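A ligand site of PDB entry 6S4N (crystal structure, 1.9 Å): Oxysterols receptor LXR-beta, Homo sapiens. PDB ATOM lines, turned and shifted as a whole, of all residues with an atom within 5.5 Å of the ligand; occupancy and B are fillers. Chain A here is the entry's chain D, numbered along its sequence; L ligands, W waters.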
ATOM      1  N   ASN A  23       8.195   5.344  10.257  1.00  0.00           N
ATOM      2  CA  ASN A  23       7.953   6.041  11.524  1.00  0.00           C
ATOM      3  C   ASN A  23       7.405   5.125  12.596  1.00  0.00           C
ATOM      4  O   ASN A  23       7.683   5.307  13.768  1.00  0.00           O
ATOM      5  CB  ASN A  23       6.977   7.209  11.340  1.00  0.00           C
ATOM      6  CG  ASN A  23       6.990   8.154  12.512  1.00  0.00           C
ATOM      7  OD1 ASN A  23       5.956   8.391  13.143  1.00  0.00           O
ATOM      8  ND2 ASN A  23       8.167   8.696  12.842  1.00  0.00           N
ATOM      9  N   SER A  26      10.425   3.507  14.166  1.00  0.00           N
ATOM     10  CA  SER A  26      11.089   4.466  15.078  1.00  0.00           C
ATOM     11  C   SER A  26      10.420   4.517  16.464  1.00  0.00           C
ATOM     12  O   SER A  26      11.092   4.667  17.485  1.00  0.00           O
ATOM     13  CB  SER A  26      10.987   5.873  14.520  1.00  0.00           C
ATOM     14  OG  SER A  26      11.642   5.977  13.267  1.00  0.00           O
ATOM     15  N   PHE A  52      22.174  15.525  26.619  1.00  0.00           N
ATOM     16  CA  PHE A  52      22.918  15.428  25.372  1.00  0.00           C
ATOM     17  C   PHE A  52      22.803  14.030  24.741  1.00  0.00           C
ATOM     18  O   PHE A  52      22.562  13.887  23.550  1.00  0.00           O
ATOM     19  CB  PHE A  52      24.378  15.793  25.621  1.00  0.00           C
ATOM     20  CG  PHE A  52      25.255  15.716  24.399  1.00  0.00           C
ATOM     21  CD1 PHE A  52      25.254  16.718  23.449  1.00  0.00           C
ATOM     22  CD2 PHE A  52      26.112  14.634  24.219  1.00  0.00           C
ATOM     23  CE1 PHE A  52      26.073  16.648  22.333  1.00  0.00           C
ATOM     24  CE2 PHE A  52      26.949  14.562  23.119  1.00  0.00           C
ATOM     25  CZ  PHE A  52      26.932  15.573  22.177  1.00  0.00           C
ATOM     26  N   PHE A  55      19.345  13.522  23.201  1.00  0.00           N
ATOM     27  CA  PHE A  55      19.182  14.181  21.908  1.00  0.00           C
ATOM     28  C   PHE A  55      19.927  13.432  20.781  1.00  0.00           C
ATOM     29  O   PHE A  55      19.361  13.277  19.675  1.00  0.00           O
ATOM     30  CB  PHE A  55      19.620  15.663  21.958  1.00  0.00           C
ATOM     31  CG  PHE A  55      18.460  16.625  21.918  1.00  0.00           C
ATOM     32  CD1 PHE A  55      17.493  16.569  22.913  1.00  0.00           C
ATOM     33  CD2 PHE A  55      18.379  17.642  20.963  1.00  0.00           C
ATOM     34  CE1 PHE A  55      16.432  17.460  22.933  1.00  0.00           C
ATOM     35  CE2 PHE A  55      17.332  18.537  20.980  1.00  0.00           C
ATOM     36  CZ  PHE A  55      16.349  18.447  21.956  1.00  0.00           C
ATOM     37  N   THR A  56      21.150  12.987  21.063  1.00  0.00           N
ATOM     38  CA  THR A  56      21.919  12.236  20.071  1.00  0.00           C
ATOM     39  C   THR A  56      21.302  10.861  19.768  1.00  0.00           C
ATOM     40  O   THR A  56      21.401  10.362  18.649  1.00  0.00           O
ATOM     41  CB  THR A  56      23.409  12.046  20.463  1.00  0.00           C
ATOM     42  OG1 THR A  56      23.516  11.345  21.713  1.00  0.00           O
ATOM     43  CG2 THR A  56      24.134  13.396  20.576  1.00  0.00           C
ATOM     44  N   LEU A  58      17.984  10.220  19.964  1.00  0.00           N
ATOM     45  CA  LEU A  58      16.849  10.565  19.080  1.00  0.00           C
ATOM     46  C   LEU A  58      17.336  10.745  17.637  1.00  0.00           C
ATOM     47  O   LEU A  58      16.685  10.269  16.707  1.00  0.00           O
ATOM     48  CB  LEU A  58      16.118  11.819  19.545  1.00  0.00           C
ATOM     49  CG  LEU A  58      15.218  11.706  20.785  1.00  0.00           C
ATOM     50  CD1 LEU A  58      14.637  13.079  21.107  1.00  0.00           C
ATOM     51  CD2 LEU A  58      14.111  10.677  20.687  1.00  0.00           C
ATOM     52  N   ALA A  59      18.480  11.412  17.473  1.00  0.00           N
ATOM     53  CA  ALA A  59      19.069  11.627  16.155  1.00  0.00           C
ATOM     54  C   ALA A  59      19.404  10.314  15.462  1.00  0.00           C
ATOM     55  O   ALA A  59      19.155  10.175  14.275  1.00  0.00           O
ATOM     56  CB  ALA A  59      20.294  12.509  16.259  1.00  0.00           C
ATOM     57  N   ILE A  61      17.899   7.416  15.926  1.00  0.00           N
ATOM     58  CA  ILE A  61      16.601   6.895  15.495  1.00  0.00           C
ATOM     59  C   ILE A  61      16.133   7.579  14.206  1.00  0.00           C
ATOM     60  O   ILE A  61      15.681   6.906  13.276  1.00  0.00           O
ATOM     61  CB  ILE A  61      15.539   7.034  16.613  1.00  0.00           C
ATOM     62  CG1 ILE A  61      15.883   6.047  17.757  1.00  0.00           C
ATOM     63  CG2 ILE A  61      14.138   6.761  16.085  1.00  0.00           C
ATOM     64  CD1 ILE A  61      15.148   6.297  19.053  1.00  0.00           C
ATOM     65  N   SER A  62      16.285   8.899  14.148  1.00  0.00           N
ATOM     66  CA  SER A  62      15.944   9.668  12.952  1.00  0.00           C
ATOM     67  C   SER A  62      16.766   9.242  11.737  1.00  0.00           C
ATOM     68  O   SER A  62      16.202   9.069  10.657  1.00  0.00           O
ATOM     69  CB  SER A  62      16.106  11.168  13.213  1.00  0.00           C
ATOM     70  OG  SER A  62      15.701  11.926  12.106  1.00  0.00           O
ATOM     71  N   GLU A  65      15.460   5.975  10.413  1.00  0.00           N
ATOM     72  CA  GLU A  65      14.212   6.268   9.696  1.00  0.00           C
ATOM     73  C   GLU A  65      14.456   6.822   8.290  1.00  0.00           C
ATOM     74  O   GLU A  65      13.775   6.438   7.345  1.00  0.00           O
ATOM     75  CB  GLU A  65      13.371   7.290  10.471  1.00  0.00           C
ATOM     76  CG  GLU A  65      11.918   7.259  10.049  1.00  0.00           C
ATOM     77  CD  GLU A  65      11.001   8.157  10.859  1.00  0.00           C
ATOM     78  OE1 GLU A  65      10.198   8.872  10.227  1.00  0.00           O
ATOM     79  OE2 GLU A  65      11.073   8.136  12.095  1.00  0.00           O
ATOM     80  N   ILE A  93      20.698  15.921   7.764  1.00  0.00           N
ATOM     81  CA  ILE A  93      20.390  17.085   8.617  1.00  0.00           C
ATOM     82  C   ILE A  93      19.170  17.865   8.098  1.00  0.00           C
ATOM     83  O   ILE A  93      18.319  18.293   8.896  1.00  0.00           O
ATOM     84  CB  ILE A  93      21.596  18.030   8.845  1.00  0.00           C
ATOM     85  CG1 ILE A  93      21.258  19.113   9.864  1.00  0.00           C
ATOM     86  CG2 ILE A  93      22.073  18.685   7.530  1.00  0.00           C
ATOM     87  CD1 ILE A  93      20.910  18.604  11.258  1.00  0.00           C
ATOM     88  N   ILE A  95      16.625  16.735   6.266  1.00  0.00           N
ATOM     89  CA  ILE A  95      15.416  15.954   6.507  1.00  0.00           C
ATOM     90  C   ILE A  95      15.038  16.018   8.002  1.00  0.00           C
ATOM     91  O   ILE A  95      13.862  16.203   8.329  1.00  0.00           O
ATOM     92  CB  ILE A  95      15.544  14.488   6.005  1.00  0.00           C
ATOM     93  CG1 ILE A  95      15.727  14.466   4.489  1.00  0.00           C
ATOM     94  CG2 ILE A  95      14.308  13.692   6.368  1.00  0.00           C
ATOM     95  CD1 ILE A  95      16.180  13.159   3.886  1.00  0.00           C
ATOM     96  N   MET A  96      16.036  15.915   8.884  1.00  0.00           N
ATOM     97  CA  MET A  96      15.800  16.101  10.327  1.00  0.00           C
ATOM     98  C   MET A  96      15.144  17.450  10.651  1.00  0.00           C
ATOM     99  O   MET A  96      14.265  17.529  11.514  1.00  0.00           O
ATOM    100  CB  MET A  96      17.099  16.014  11.122  1.00  0.00           C
ATOM    101  CG  MET A  96      17.632  14.613  11.293  1.00  0.00           C
ATOM    102  SD  MET A  96      19.195  14.667  12.172  1.00  0.00           S
ATOM    103  CE  MET A  96      19.575  12.929  12.229  1.00  0.00           C
ATOM    104  N   LEU A  97      15.595  18.496   9.963  1.00  0.00           N
ATOM    105  CA  LEU A  97      15.014  19.833  10.143  1.00  0.00           C
ATOM    106  C   LEU A  97      13.571  19.919   9.627  1.00  0.00           C
ATOM    107  O   LEU A  97      12.728  20.559  10.265  1.00  0.00           O
ATOM    108  CB  LEU A  97      15.890  20.885   9.462  1.00  0.00           C
ATOM    109  CG  LEU A  97      17.240  21.093  10.145  1.00  0.00           C
ATOM    110  CD1 LEU A  97      18.225  21.727   9.186  1.00  0.00           C
ATOM    111  CD2 LEU A  97      17.090  21.909  11.416  1.00  0.00           C
ATOM    112  N   GLU A  99      11.534  17.329   9.521  1.00  0.00           N
ATOM    113  CA  GLU A  99      10.801  16.523  10.485  1.00  0.00           C
ATOM    114  C   GLU A  99      10.618  17.266  11.827  1.00  0.00           C
ATOM    115  O   GLU A  99       9.573  17.138  12.471  1.00  0.00           O
ATOM    116  CB  GLU A  99      11.469  15.164  10.688  1.00  0.00           C
ATOM    117  CG  GLU A  99      11.434  14.256   9.447  1.00  0.00           C
ATOM    118  CD  GLU A  99      10.057  13.699   9.101  1.00  0.00           C
ATOM    119  OE1 GLU A  99       9.068  13.981   9.801  1.00  0.00           O
ATOM    120  OE2 GLU A  99       9.968  12.956   8.083  1.00  0.00           O
ATOM    121  N   THR A 100      11.624  18.033  12.236  1.00  0.00           N
ATOM    122  CA  THR A 100      11.533  18.915  13.393  1.00  0.00           C
ATOM    123  C   THR A 100      10.419  19.968  13.208  1.00  0.00           C
ATOM    124  O   THR A 100       9.559  20.162  14.083  1.00  0.00           O
ATOM    125  CB  THR A 100      12.905  19.580  13.678  1.00  0.00           C
ATOM    126  OG1 THR A 100      13.840  18.580  14.082  1.00  0.00           O
ATOM    127  CG2 THR A 100      12.819  20.621  14.789  1.00  0.00           C
ATOM    128  N   ARG A 103       6.941  18.604  13.554  1.00  0.00           N
ATOM    129  CA  ARG A 103       6.578  18.319  14.940  1.00  0.00           C
ATOM    130  C   ARG A 103       6.437  19.573  15.833  1.00  0.00           C
ATOM    131  O   ARG A 103       6.262  19.438  17.043  1.00  0.00           O
ATOM    132  CB  ARG A 103       7.600  17.356  15.517  1.00  0.00           C
ATOM    133  CG  ARG A 103       7.500  15.953  14.923  1.00  0.00           C
ATOM    134  CD  ARG A 103       8.801  15.155  15.022  1.00  0.00           C
ATOM    135  NE  ARG A 103       8.580  13.779  14.590  1.00  0.00           N
ATOM    136  CZ  ARG A 103       8.460  13.371  13.311  1.00  0.00           C
ATOM    137  NH1 ARG A 103       8.529  14.222  12.292  1.00  0.00           N
ATOM    138  NH2 ARG A 103       8.259  12.085  13.056  1.00  0.00           N
ATOM    139  N   THR A 112       7.707  18.165  19.492  1.00  0.00           N
ATOM    140  CA  THR A 112       7.443  16.833  20.044  1.00  0.00           C
ATOM    141  C   THR A 112       8.039  15.714  19.204  1.00  0.00           C
ATOM    142  O   THR A 112       7.613  15.499  18.072  1.00  0.00           O
ATOM    143  CB  THR A 112       5.937  16.578  20.182  1.00  0.00           C
ATOM    144  OG1 THR A 112       5.339  17.598  20.979  1.00  0.00           O
ATOM    145  CG2 THR A 112       5.665  15.199  20.830  1.00  0.00           C
ATOM    146  N   PHE A 113       9.009  14.999  19.769  1.00  0.00           N
ATOM    147  CA  PHE A 113       9.599  13.830  19.110  1.00  0.00           C
ATOM    148  C   PHE A 113       9.067  12.528  19.712  1.00  0.00           C
ATOM    149  O   PHE A 113       8.886  12.457  20.913  1.00  0.00           O
ATOM    150  CB  PHE A 113      11.124  13.858  19.207  1.00  0.00           C
ATOM    151  CG  PHE A 113      11.733  15.118  18.635  1.00  0.00           C
ATOM    152  CD1 PHE A 113      11.816  15.292  17.255  1.00  0.00           C
ATOM    153  CD2 PHE A 113      12.194  16.122  19.477  1.00  0.00           C
ATOM    154  CE1 PHE A 113      12.361  16.442  16.729  1.00  0.00           C
ATOM    155  CE2 PHE A 113      12.749  17.289  18.954  1.00  0.00           C
ATOM    156  CZ  PHE A 113      12.837  17.447  17.578  1.00  0.00           C
ATOM    157  N   LEU A 114       8.815  11.549  18.866  1.00  0.00           N
ATOM    158  CA  LEU A 114       8.316  10.222  19.276  1.00  0.00           C
ATOM    159  C   LEU A 114       7.038  10.277  20.131  1.00  0.00           C
ATOM    160  O   LEU A 114       6.840   9.486  21.064  1.00  0.00           O
ATOM    161  CB  LEU A 114       9.425   9.445  19.979  1.00  0.00           C
ATOM    162  CG  LEU A 114      10.614   9.106  19.086  1.00  0.00           C
ATOM    163  CD1 LEU A 114      11.652   8.314  19.868  1.00  0.00           C
ATOM    164  CD2 LEU A 114      10.247   8.302  17.829  1.00  0.00           C
ATOM    165  N   LYS A 115       6.108  11.149  19.760  1.00  0.00           N
ATOM    166  CA  LYS A 115       4.820  11.273  20.455  1.00  0.00           C
ATOM    167  C   LYS A 115       4.713  11.937  21.762  1.00  0.00           C
ATOM    168  O   LYS A 115       3.715  12.619  22.010  1.00  0.00           O
ATOM    169  CB  LYS A 115       3.594  10.556  19.852  1.00  0.00           C
ATOM    170  CG  LYS A 115       3.922   9.376  18.955  1.00  0.00           C
ATOM    171  N   PHE A 124      16.296  22.680  24.201  1.00  0.00           N
ATOM    172  CA  PHE A 124      17.330  22.509  23.167  1.00  0.00           C
ATOM    173  C   PHE A 124      18.685  23.020  23.655  1.00  0.00           C
ATOM    174  O   PHE A 124      19.704  22.367  23.444  1.00  0.00           O
ATOM    175  CB  PHE A 124      16.932  23.258  21.870  1.00  0.00           C
ATOM    176  CG  PHE A 124      16.061  22.456  20.935  1.00  0.00           C
ATOM    177  CD1 PHE A 124      14.827  21.960  21.343  1.00  0.00           C
ATOM    178  CD2 PHE A 124      16.403  22.327  19.602  1.00  0.00           C
ATOM    179  CE1 PHE A 124      14.027  21.220  20.486  1.00  0.00           C
ATOM    180  CE2 PHE A 124      15.608  21.625  18.712  1.00  0.00           C
ATOM    181  CZ  PHE A 124      14.417  21.060  19.162  1.00  0.00           C
ATOM    182  N   LEU A 129      22.849  22.337  22.549  1.00  0.00           N
ATOM    183  CA  LEU A 129      22.880  23.119  21.289  1.00  0.00           C
ATOM    184  C   LEU A 129      23.101  24.615  21.576  1.00  0.00           C
ATOM    185  O   LEU A 129      22.702  25.115  22.602  1.00  0.00           O
ATOM    186  CB  LEU A 129      21.591  22.905  20.478  1.00  0.00           C
ATOM    187  CG  LEU A 129      21.483  21.634  19.626  1.00  0.00           C
ATOM    188  CD1 LEU A 129      21.525  20.353  20.438  1.00  0.00           C
ATOM    189  CD2 LEU A 129      20.207  21.691  18.782  1.00  0.00           C
ATOM    190  N   PHE A 133      22.189  28.107  16.414  1.00  0.00           N
ATOM    191  CA  PHE A 133      21.510  27.034  15.663  1.00  0.00           C
ATOM    192  C   PHE A 133      20.042  26.897  16.091  1.00  0.00           C
ATOM    193  O   PHE A 133      19.174  26.734  15.249  1.00  0.00           O
ATOM    194  CB  PHE A 133      22.272  25.711  15.863  1.00  0.00           C
ATOM    195  CG  PHE A 133      21.748  24.553  15.042  1.00  0.00           C
ATOM    196  CD1 PHE A 133      21.319  24.704  13.728  1.00  0.00           C
ATOM    197  CD2 PHE A 133      21.775  23.267  15.585  1.00  0.00           C
ATOM    198  CE1 PHE A 133      20.878  23.598  12.999  1.00  0.00           C
ATOM    199  CE2 PHE A 133      21.332  22.174  14.861  1.00  0.00           C
ATOM    200  CZ  PHE A 133      20.878  22.338  13.559  1.00  0.00           C
ATOM    201  N   ILE A 137      16.435  27.162  13.827  1.00  0.00           N
ATOM    202  CA  ILE A 137      15.573  25.964  13.823  1.00  0.00           C
ATOM    203  C   ILE A 137      14.127  26.351  14.095  1.00  0.00           C
ATOM    204  O   ILE A 137      13.219  25.916  13.390  1.00  0.00           O
ATOM    205  CB  ILE A 137      16.016  24.907  14.864  1.00  0.00           C
ATOM    206  CG1 ILE A 137      17.332  24.229  14.389  1.00  0.00           C
ATOM    207  CG2 ILE A 137      14.929  23.839  15.074  1.00  0.00           C
ATOM    208  CD1 ILE A 137      18.015  23.464  15.494  1.00  0.00           C
ATOM    209  N   HIS A 219      24.323  24.248  11.020  1.00  0.00           N
ATOM    210  CA  HIS A 219      24.537  22.965  11.698  1.00  0.00           C
ATOM    211  C   HIS A 219      26.015  22.550  11.692  1.00  0.00           C
ATOM    212  O   HIS A 219      26.517  22.045  12.704  1.00  0.00           O
ATOM    213  CB  HIS A 219      23.688  21.875  11.053  1.00  0.00           C
ATOM    214  CG  HIS A 219      23.961  20.516  11.603  1.00  0.00           C
ATOM    215  ND1 HIS A 219      24.763  19.604  10.961  1.00  0.00           N
ATOM    216  CD2 HIS A 219      23.536  19.917  12.748  1.00  0.00           C
ATOM    217  CE1 HIS A 219      24.829  18.493  11.671  1.00  0.00           C
ATOM    218  NE2 HIS A 219      24.090  18.659  12.765  1.00  0.00           N
ATOM    219  N   GLN A 222      27.626  24.338  14.400  1.00  0.00           N
ATOM    220  CA  GLN A 222      27.249  23.655  15.645  1.00  0.00           C
ATOM    221  C   GLN A 222      28.127  22.430  15.902  1.00  0.00           C
ATOM    222  O   GLN A 222      28.596  22.237  17.027  1.00  0.00           O
ATOM    223  CB  GLN A 222      25.763  23.258  15.622  1.00  0.00           C
ATOM    224  CG  GLN A 222      25.317  22.311  16.711  1.00  0.00           C
ATOM    225  CD  GLN A 222      25.271  22.992  18.050  1.00  0.00           C
ATOM    226  OE1 GLN A 222      26.260  23.037  18.788  1.00  0.00           O
ATOM    227  NE2 GLN A 222      24.141  23.603  18.365  1.00  0.00           N
ATOM    228  N   VAL A 223      28.336  21.608  14.874  1.00  0.00           N
ATOM    229  CA  VAL A 223      29.166  20.402  14.975  1.00  0.00           C
ATOM    230  C   VAL A 223      30.611  20.783  15.332  1.00  0.00           C
ATOM    231  O   VAL A 223      31.223  20.148  16.205  1.00  0.00           O
ATOM    232  CB  VAL A 223      29.105  19.554  13.686  1.00  0.00           C
ATOM    233  CG1 VAL A 223      30.121  18.410  13.714  1.00  0.00           C
ATOM    234  CG2 VAL A 223      27.716  18.964  13.517  1.00  0.00           C
ATOM    235  N   LEU A 226      30.883  21.754  19.066  1.00  0.00           N
ATOM    236  CA  LEU A 226      30.943  20.574  19.929  1.00  0.00           C
ATOM    237  C   LEU A 226      32.345  19.988  20.017  1.00  0.00           C
ATOM    238  O   LEU A 226      32.752  19.510  21.086  1.00  0.00           O
ATOM    239  CB  LEU A 226      29.969  19.499  19.453  1.00  0.00           C
ATOM    240  CG  LEU A 226      28.483  19.855  19.485  1.00  0.00           C
ATOM    241  CD1 LEU A 226      27.664  18.746  18.847  1.00  0.00           C
ATOM    242  CD2 LEU A 226      27.989  20.125  20.906  1.00  0.00           C
ATOM    243  N   LEU A 233      30.280  12.881  19.565  1.00  0.00           N
ATOM    244  CA  LEU A 233      29.091  12.321  18.960  1.00  0.00           C
ATOM    245  C   LEU A 233      29.215  10.808  18.911  1.00  0.00           C
ATOM    246  O   LEU A 233      30.325  10.289  18.763  1.00  0.00           O
ATOM    247  CB  LEU A 233      28.902  12.863  17.537  1.00  0.00           C
ATOM    248  CG  LEU A 233      28.580  14.344  17.379  1.00  0.00           C
ATOM    249  CD1 LEU A 233      28.594  14.686  15.889  1.00  0.00           C
ATOM    250  CD2 LEU A 233      27.217  14.671  17.988  1.00  0.00           C
ATOM    251  N   LEU A 237      26.589   9.325  14.011  1.00  0.00           N
ATOM    252  CA  LEU A 237      26.490  10.771  13.792  1.00  0.00           C
ATOM    253  C   LEU A 237      27.841  11.394  13.459  1.00  0.00           C
ATOM    254  O   LEU A 237      27.918  12.304  12.632  1.00  0.00           O
ATOM    255  CB  LEU A 237      25.861  11.480  15.005  1.00  0.00           C
ATOM    256  CG  LEU A 237      24.493  10.990  15.462  1.00  0.00           C
ATOM    257  CD1 LEU A 237      24.022  11.822  16.630  1.00  0.00           C
ATOM    258  CD2 LEU A 237      23.475  11.016  14.332  1.00  0.00           C
ATOM    259  N   TRP A 241      28.553  13.558  10.179  1.00  0.00           N
ATOM    260  CA  TRP A 241      28.742  14.993  10.443  1.00  0.00           C
ATOM    261  C   TRP A 241      30.159  15.515  10.702  1.00  0.00           C
ATOM    262  O   TRP A 241      30.437  16.680  10.384  1.00  0.00           O
ATOM    263  CB  TRP A 241      27.820  15.425  11.567  1.00  0.00           C
ATOM    264  CG  TRP A 241      26.363  15.325  11.221  1.00  0.00           C
ATOM    265  CD1 TRP A 241      25.802  15.380   9.976  1.00  0.00           C
ATOM    266  CD2 TRP A 241      25.275  15.203  12.139  1.00  0.00           C
ATOM    267  NE1 TRP A 241      24.440  15.258  10.054  1.00  0.00           N
ATOM    268  CE2 TRP A 241      24.086  15.158  11.369  1.00  0.00           C
ATOM    269  CE3 TRP A 241      25.181  15.129  13.534  1.00  0.00           C
ATOM    270  CZ2 TRP A 241      22.828  15.031  11.951  1.00  0.00           C
ATOM    271  CZ3 TRP A 241      23.923  15.002  14.115  1.00  0.00           C
ATOM    272  CH2 TRP A 241      22.759  14.958  13.317  1.00  0.00           C
HETATM  273  C1  LIG L   1      24.079  17.706  19.080  1.00  0.00           C
HETATM  274  C2  LIG L   1      23.986  16.944  17.751  1.00  0.00           C
HETATM  275  C3  LIG L   1      24.927  17.626  16.744  1.00  0.00           C
HETATM  276  C4  LIG L   1      20.221  16.597  17.284  1.00  0.00           C
HETATM  277  C5  LIG L   1      20.169  17.705  16.471  1.00  0.00           C
HETATM  278  C6  LIG L   1      19.071  18.391  15.768  1.00  0.00           C
HETATM  279  C7  LIG L   1      18.065  19.073  16.486  1.00  0.00           C
HETATM  280  C8  LIG L   1      17.058  19.726  15.779  1.00  0.00           C
HETATM  281  C9  LIG L   1      17.057  19.716  14.383  1.00  0.00           C
HETATM  282  C10 LIG L   1      18.065  19.056  13.672  1.00  0.00           C
HETATM  283  C11 LIG L   1      19.064  18.398  14.368  1.00  0.00           C
HETATM  284  O1  LIG L   1      22.258  17.932  15.001  1.00  0.00           O
HETATM  285  N1  LIG L   1      19.146  15.825  17.754  1.00  0.00           N
HETATM  286  C12 LIG L   1      17.783  15.817  17.206  1.00  0.00           C
HETATM  287  C13 LIG L   1      17.753  15.183  15.805  1.00  0.00           C
HETATM  288  C14 LIG L   1      16.329  15.271  15.274  1.00  0.00           C
HETATM  289  C15 LIG L   1      16.865  15.100  18.195  1.00  0.00           C
HETATM  290  N2  LIG L   1      14.200  12.770  16.801  1.00  0.00           N
HETATM  291  C16 LIG L   1      13.338  11.788  16.565  1.00  0.00           C
HETATM  292  C17 LIG L   1      10.228  11.094  15.555  1.00  0.00           C
HETATM  293  C18 LIG L   1      12.777  12.795  14.463  1.00  0.00           C
HETATM  294  C19 LIG L   1      13.685  13.813  14.731  1.00  0.00           C
HETATM  295  N3  LIG L   1      22.572  17.051  17.354  1.00  0.00           N
HETATM  296  C20 LIG L   1      21.549  16.268  17.762  1.00  0.00           C
HETATM  297  O2  LIG L   1      21.714  15.336  18.527  1.00  0.00           O
HETATM  298  S1  LIG L   1      21.864  18.188  16.336  1.00  0.00           S
HETATM  299  O3  LIG L   1      22.042  19.456  16.940  1.00  0.00           O
HETATM  300  N4  LIG L   1      15.345  14.760  16.273  1.00  0.00           N
HETATM  301  C21 LIG L   1      15.429  15.215  17.687  1.00  0.00           C
HETATM  302  C22 LIG L   1      14.416  13.766  15.932  1.00  0.00           C
HETATM  303  C23 LIG L   1      12.599  11.777  15.390  1.00  0.00           C
HETATM  304  C24 LIG L   1      11.612  10.681  15.096  1.00  0.00           C
HETATM  305  O4  LIG L   1      10.039  12.035  16.290  1.00  0.00           O
HETATM  306  O5  LIG L   1       9.169  10.398  15.131  1.00  0.00           O
HETATM  307 CL1  LIG L   1      13.854  15.060  13.533  1.00  0.00          CL
HETATM  308  O   HOH W   1       6.792  11.143  16.220  1.00  0.00           O
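Water W1 lies within hydrogen-bond range of an oxygen (O5) of the ligand (2.7 Å) and the backbone NH (N) of Leu 114 (3.4 Å).
NH2 of Arg 103 lies close to ND2 of Asn 23, 3.4 Å away.
NH1 of Arg 103 is in salt-bridge range of OE1 of Glu 99 (2.6 Å).
N of Thr 112 lies within hydrogen-bond range of O of Arg 103, 3.1 Å away.
The side-chain amide nitrogen of Asn 23 sits at hydrogen-bond distance from the side-chain carboxylate of Glu 65.
The backbone carbonyl oxygen (O) of Met 96 is in hydrogen-bond range of the side-chain hydroxyl (OG1) of Thr 100.
The backbone NH (N) of Leu 129 sits at hydrogen-bond distance from the backbone carbonyl oxygen (O) of Phe 124 (3.3 Å).
The side-chain hydroxyl (OG1) of Thr 56 sits at hydrogen-bond distance from the backbone carbonyl oxygen (O) of Phe 52, 3.3 Å away.
OE2 of Glu 65 sits at hydrogen-bond distance from OG of Ser 26.
NH2 of Arg 103 is in salt-bridge range of O5 of the ligand, 2.8 Å away.
The backbone NH (N) of Leu 114 sits at hydrogen-bond distance from an oxygen (O4) of the ligand (2.9 Å).
A ring nitrogen (NE2) of His 219 is in hydrogen-bond range of an oxygen (O1) of the ligand (3.0 Å).
O5 of the ligand sits at hydrogen-bond distance from ND2 of Asn 23 (3.0 Å).
A nitrogen (N1) of the ligand is in hydrogen-bond range of the backbone carbonyl oxygen (O) of Phe 55.
Merely in contact with the ligand: Phe 52 (3.96 Å), Thr 56 (3.5 Å), Leu 58 (3.5 Å), Ala 59 (3.7 Å), Ser 62 (3.8 Å), Glu 65 (3.97 Å), Ile 93 (3.6 Å), Met 96 (3.2 Å), Leu 97 (3.7 Å), Glu 99 (3.7 Å), Thr 100 (3.4 Å), Phe 113 (3.3 Å), Phe 124 (3.8 Å), Leu 129 (3.4 Å), Phe 133 (3.5 Å), Ile 137 (3.9 Å), Leu 226 (3.6 Å), Leu 233 (3.9 Å) and Trp 241 (3.5 Å).
24 residues have an atom within 4 Å of the ligand: Asn 23, Phe 52, Phe 55, Thr 56, Leu 58, Ala 59, Ser 62, Glu 65, Ile 93, Met 96, Leu 97, Glu 99, Thr 100, Arg 103, Phe 113, Leu 114, Phe 124, Leu 129, Phe 133, Ile 137, His 219, Leu 226, Leu 233 and Trp 241.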
